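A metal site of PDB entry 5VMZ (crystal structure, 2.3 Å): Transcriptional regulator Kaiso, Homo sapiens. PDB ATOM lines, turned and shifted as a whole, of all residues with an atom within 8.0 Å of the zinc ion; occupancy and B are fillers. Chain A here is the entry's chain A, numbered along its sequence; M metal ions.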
ATOM      1  N   PRO A  53     -31.232   8.062 -32.765  1.00  0.00           N
ATOM      2  CA  PRO A  53     -31.738   8.433 -31.432  1.00  0.00           C
ATOM      3  C   PRO A  53     -31.817   7.240 -30.494  1.00  0.00           C
ATOM      4  O   PRO A  53     -32.273   6.183 -30.928  1.00  0.00           O
ATOM      5  CB  PRO A  53     -33.141   8.994 -31.720  1.00  0.00           C
ATOM      6  CG  PRO A  53     -33.575   8.290 -32.988  1.00  0.00           C
ATOM      7  CD  PRO A  53     -32.301   8.033 -33.784  1.00  0.00           C
ATOM      8  N   CYS A  54     -31.355   7.393 -29.243  1.00  0.00           N
ATOM      9  CA  CYS A  54     -31.488   6.334 -28.239  1.00  0.00           C
ATOM     10  C   CYS A  54     -32.945   6.030 -28.043  1.00  0.00           C
ATOM     11  O   CYS A  54     -33.743   6.940 -27.846  1.00  0.00           O
ATOM     12  CB  CYS A  54     -30.873   6.705 -26.891  1.00  0.00           C
ATOM     13  SG  CYS A  54     -31.190   5.454 -25.567  1.00  0.00           S
ATOM     14  N   ARG A  55     -33.304   4.757 -28.084  1.00  0.00           N
ATOM     15  CA  ARG A  55     -34.711   4.419 -27.944  1.00  0.00           C
ATOM     16  C   ARG A  55     -35.115   4.213 -26.480  1.00  0.00           C
ATOM     17  O   ARG A  55     -36.118   3.565 -26.195  1.00  0.00           O
ATOM     18  CB  ARG A  55     -35.036   3.181 -28.777  1.00  0.00           C
ATOM     19  CG  ARG A  55     -34.234   3.117 -30.074  1.00  0.00           C
ATOM     20  CD  ARG A  55     -33.806   1.686 -30.298  1.00  0.00           C
ATOM     21  NE  ARG A  55     -32.675   1.527 -31.213  1.00  0.00           N
ATOM     22  CZ  ARG A  55     -32.792   1.267 -32.506  1.00  0.00           C
ATOM     23  NH1 ARG A  55     -33.989   1.158 -33.061  1.00  0.00           N
ATOM     24  NH2 ARG A  55     -31.704   1.107 -33.252  1.00  0.00           N
ATOM     25  N   TYR A  56     -34.333   4.763 -25.559  1.00  0.00           N
ATOM     26  CA  TYR A  56     -34.627   4.643 -24.127  1.00  0.00           C
ATOM     27  C   TYR A  56     -34.563   5.981 -23.429  1.00  0.00           C
ATOM     28  O   TYR A  56     -35.150   6.154 -22.347  1.00  0.00           O
ATOM     29  CB  TYR A  56     -33.654   3.682 -23.440  1.00  0.00           C
ATOM     30  CG  TYR A  56     -33.659   2.301 -23.997  1.00  0.00           C
ATOM     31  CD1 TYR A  56     -34.495   1.315 -23.470  1.00  0.00           C
ATOM     32  CD2 TYR A  56     -32.836   1.965 -25.059  1.00  0.00           C
ATOM     33  CE1 TYR A  56     -34.500   0.041 -23.998  1.00  0.00           C
ATOM     34  CE2 TYR A  56     -32.836   0.704 -25.586  1.00  0.00           C
ATOM     35  CZ  TYR A  56     -33.650  -0.254 -25.052  1.00  0.00           C
ATOM     36  OH  TYR A  56     -33.631  -1.522 -25.593  1.00  0.00           O
ATOM     37  N   CYS A  57     -33.841   6.925 -24.028  1.00  0.00           N
ATOM     38  CA  CYS A  57     -33.817   8.274 -23.492  1.00  0.00           C
ATOM     39  C   CYS A  57     -33.756   9.289 -24.638  1.00  0.00           C
ATOM     40  O   CYS A  57     -34.116   8.986 -25.778  1.00  0.00           O
ATOM     41  CB  CYS A  57     -32.651   8.463 -22.511  1.00  0.00           C
ATOM     42  SG  CYS A  57     -31.025   8.545 -23.306  1.00  0.00           S
ATOM     43  N   GLU A  58     -33.311  10.506 -24.343  1.00  0.00           N
ATOM     44  CA  GLU A  58     -33.416  11.591 -25.312  1.00  0.00           C
ATOM     45  C   GLU A  58     -32.183  11.687 -26.201  1.00  0.00           C
ATOM     46  O   GLU A  58     -32.265  12.210 -27.301  1.00  0.00           O
ATOM     47  CB  GLU A  58     -33.679  12.922 -24.588  1.00  0.00           C
ATOM     48  CG  GLU A  58     -32.519  13.420 -23.715  1.00  0.00           C
ATOM     49  CD  GLU A  58     -32.326  12.606 -22.435  1.00  0.00           C
ATOM     50  OE1 GLU A  58     -33.253  11.879 -22.024  1.00  0.00           O
ATOM     51  OE2 GLU A  58     -31.227  12.685 -21.832  1.00  0.00           O
ATOM     52  N   LYS A  59     -31.058  11.158 -25.744  1.00  0.00           N
ATOM     53  CA  LYS A  59     -29.781  11.309 -26.447  1.00  0.00           C
ATOM     54  C   LYS A  59     -29.834  10.860 -27.913  1.00  0.00           C
ATOM     55  O   LYS A  59     -30.451   9.858 -28.269  1.00  0.00           O
ATOM     56  CB  LYS A  59     -28.690  10.535 -25.705  1.00  0.00           C
ATOM     57  CG  LYS A  59     -28.424  11.060 -24.300  1.00  0.00           C
ATOM     58  CD  LYS A  59     -27.230  10.354 -23.655  1.00  0.00           C
ATOM     59  CE  LYS A  59     -26.981  10.862 -22.243  1.00  0.00           C
ATOM     60  NZ  LYS A  59     -28.205  10.762 -21.369  1.00  0.00           N
ATOM     61  N   VAL A  60     -29.176  11.644 -28.763  1.00  0.00           N
ATOM     62  CA  VAL A  60     -29.094  11.315 -30.177  1.00  0.00           C
ATOM     63  C   VAL A  60     -27.622  11.145 -30.566  1.00  0.00           C
ATOM     64  O   VAL A  60     -26.759  11.846 -30.045  1.00  0.00           O
ATOM     65  CB  VAL A  60     -29.775  12.414 -31.008  1.00  0.00           C
ATOM     66  CG1 VAL A  60     -29.636  12.148 -32.484  1.00  0.00           C
ATOM     67  CG2 VAL A  60     -31.270  12.502 -30.606  1.00  0.00           C
ATOM     68  N   PHE A  61     -27.320  10.182 -31.439  1.00  0.00           N
ATOM     69  CA  PHE A  61     -25.938   9.896 -31.818  1.00  0.00           C
ATOM     70  C   PHE A  61     -25.736  10.000 -33.314  1.00  0.00           C
ATOM     71  O   PHE A  61     -26.660   9.740 -34.082  1.00  0.00           O
ATOM     72  CB  PHE A  61     -25.530   8.494 -31.326  1.00  0.00           C
ATOM     73  CG  PHE A  61     -25.649   8.326 -29.845  1.00  0.00           C
ATOM     74  CD1 PHE A  61     -26.850   7.934 -29.274  1.00  0.00           C
ATOM     75  CD2 PHE A  61     -24.567   8.575 -29.013  1.00  0.00           C
ATOM     76  CE1 PHE A  61     -26.964   7.781 -27.905  1.00  0.00           C
ATOM     77  CE2 PHE A  61     -24.663   8.438 -27.651  1.00  0.00           C
ATOM     78  CZ  PHE A  61     -25.868   8.040 -27.087  1.00  0.00           C
ATOM     79  N   ARG A  67     -24.722   4.728 -30.716  1.00  0.00           N
ATOM     80  CA  ARG A  67     -26.013   4.516 -30.121  1.00  0.00           C
ATOM     81  C   ARG A  67     -26.127   3.101 -29.541  1.00  0.00           C
ATOM     82  O   ARG A  67     -26.587   2.917 -28.409  1.00  0.00           O
ATOM     83  CB  ARG A  67     -27.146   4.756 -31.120  1.00  0.00           C
ATOM     84  CG  ARG A  67     -28.465   4.259 -30.566  1.00  0.00           C
ATOM     85  CD  ARG A  67     -29.618   4.506 -31.481  1.00  0.00           C
ATOM     86  NE  ARG A  67     -29.491   3.751 -32.711  1.00  0.00           N
ATOM     87  CZ  ARG A  67     -30.423   3.741 -33.658  1.00  0.00           C
ATOM     88  NH1 ARG A  67     -31.537   4.428 -33.468  1.00  0.00           N
ATOM     89  NH2 ARG A  67     -30.252   3.042 -34.774  1.00  0.00           N
ATOM     90  N   HIS A  70     -24.320   2.733 -26.368  1.00  0.00           N
ATOM     91  CA  HIS A  70     -25.069   3.468 -25.368  1.00  0.00           C
ATOM     92  C   HIS A  70     -26.302   2.702 -24.896  1.00  0.00           C
ATOM     93  O   HIS A  70     -26.601   2.651 -23.704  1.00  0.00           O
ATOM     94  CB  HIS A  70     -25.508   4.822 -25.917  1.00  0.00           C
ATOM     95  CG  HIS A  70     -26.525   5.508 -25.069  1.00  0.00           C
ATOM     96  ND1 HIS A  70     -26.199   6.128 -23.880  1.00  0.00           N
ATOM     97  CD2 HIS A  70     -27.863   5.690 -25.237  1.00  0.00           C
ATOM     98  CE1 HIS A  70     -27.289   6.660 -23.354  1.00  0.00           C
ATOM     99  NE2 HIS A  70     -28.304   6.414 -24.157  1.00  0.00           N
ATOM    100  N   GLU A  71     -27.030   2.100 -25.832  1.00  0.00           N
ATOM    101  CA  GLU A  71     -28.217   1.341 -25.452  1.00  0.00           C
ATOM    102  C   GLU A  71     -27.901   0.084 -24.654  1.00  0.00           C
ATOM    103  O   GLU A  71     -28.699  -0.324 -23.811  1.00  0.00           O
ATOM    104  CB  GLU A  71     -29.029   0.986 -26.702  1.00  0.00           C
ATOM    105  CG  GLU A  71     -29.599   2.227 -27.381  1.00  0.00           C
ATOM    106  CD  GLU A  71     -30.515   1.881 -28.518  1.00  0.00           C
ATOM    107  OE1 GLU A  71     -30.335   0.801 -29.104  1.00  0.00           O
ATOM    108  OE2 GLU A  71     -31.416   2.698 -28.812  1.00  0.00           O
ATOM    109  N   ILE A  72     -26.738  -0.507 -24.891  1.00  0.00           N
ATOM    110  CA  ILE A  72     -26.340  -1.667 -24.098  1.00  0.00           C
ATOM    111  C   ILE A  72     -26.262  -1.289 -22.619  1.00  0.00           C
ATOM    112  O   ILE A  72     -26.658  -2.064 -21.746  1.00  0.00           O
ATOM    113  CB  ILE A  72     -25.000  -2.247 -24.589  1.00  0.00           C
ATOM    114  CG1 ILE A  72     -25.256  -3.231 -25.713  1.00  0.00           C
ATOM    115  CG2 ILE A  72     -24.270  -2.983 -23.460  1.00  0.00           C
ATOM    116  CD1 ILE A  72     -26.023  -4.474 -25.248  1.00  0.00           C
ATOM    117  N   HIS A  73     -25.795  -0.073 -22.345  1.00  0.00           N
ATOM    118  CA  HIS A  73     -25.802   0.471 -20.983  1.00  0.00           C
ATOM    119  C   HIS A  73     -27.189   0.556 -20.382  1.00  0.00           C
ATOM    120  O   HIS A  73     -27.330   0.442 -19.176  1.00  0.00           O
ATOM    121  CB  HIS A  73     -25.162   1.852 -20.959  1.00  0.00           C
ATOM    122  CG  HIS A  73     -23.671   1.835 -21.034  1.00  0.00           C
ATOM    123  ND1 HIS A  73     -22.985   1.831 -22.232  1.00  0.00           N
ATOM    124  CD2 HIS A  73     -22.725   1.800 -20.067  1.00  0.00           C
ATOM    125  CE1 HIS A  73     -21.683   1.799 -22.005  1.00  0.00           C
ATOM    126  NE2 HIS A  73     -21.505   1.782 -20.696  1.00  0.00           N
ATOM    127  N   HIS A  74     -28.211   0.832 -21.204  1.00  0.00           N
ATOM    128  CA  HIS A  74     -29.576   0.865 -20.675  1.00  0.00           C
ATOM    129  C   HIS A  74     -30.040  -0.536 -20.246  1.00  0.00           C
ATOM    130  O   HIS A  74     -30.724  -0.688 -19.227  1.00  0.00           O
ATOM    131  CB  HIS A  74     -30.556   1.433 -21.717  1.00  0.00           C
ATOM    132  CG  HIS A  74     -30.599   2.938 -21.793  1.00  0.00           C
ATOM    133  ND1 HIS A  74     -31.202   3.715 -20.827  1.00  0.00           N
ATOM    134  CD2 HIS A  74     -30.162   3.790 -22.750  1.00  0.00           C
ATOM    135  CE1 HIS A  74     -31.112   4.989 -21.176  1.00  0.00           C
ATOM    136  NE2 HIS A  74     -30.491   5.064 -22.338  1.00  0.00           N
HETATM  137 ZN    ZN M   1     -30.272   6.449 -23.830  1.00  0.00          ZN
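Within 4 Å of the zinc ion: Cys 54, Cys 57, His 70 and His 74.
N of Tyr 56 sits close to SG of Cys 54, 3.2 Å away.
O of Lys 59 lies within hydrogen-bond range of N of Cys 54 (2.8 Å).
N of Lys 59 lies close to SG of Cys 57, at 3.6 Å.
The zinc ion is bound by NE2 of His 70 (2.0 Å).
NE2 of His 74 is bound to the zinc ion (2.0 Å).
SG of Cys 54 is bound to the zinc ion (2.2 Å).
The zinc ion is bound by SG of Cys 57, at 2.3 Å.
The zinc ion has four donor atoms within binding distance.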
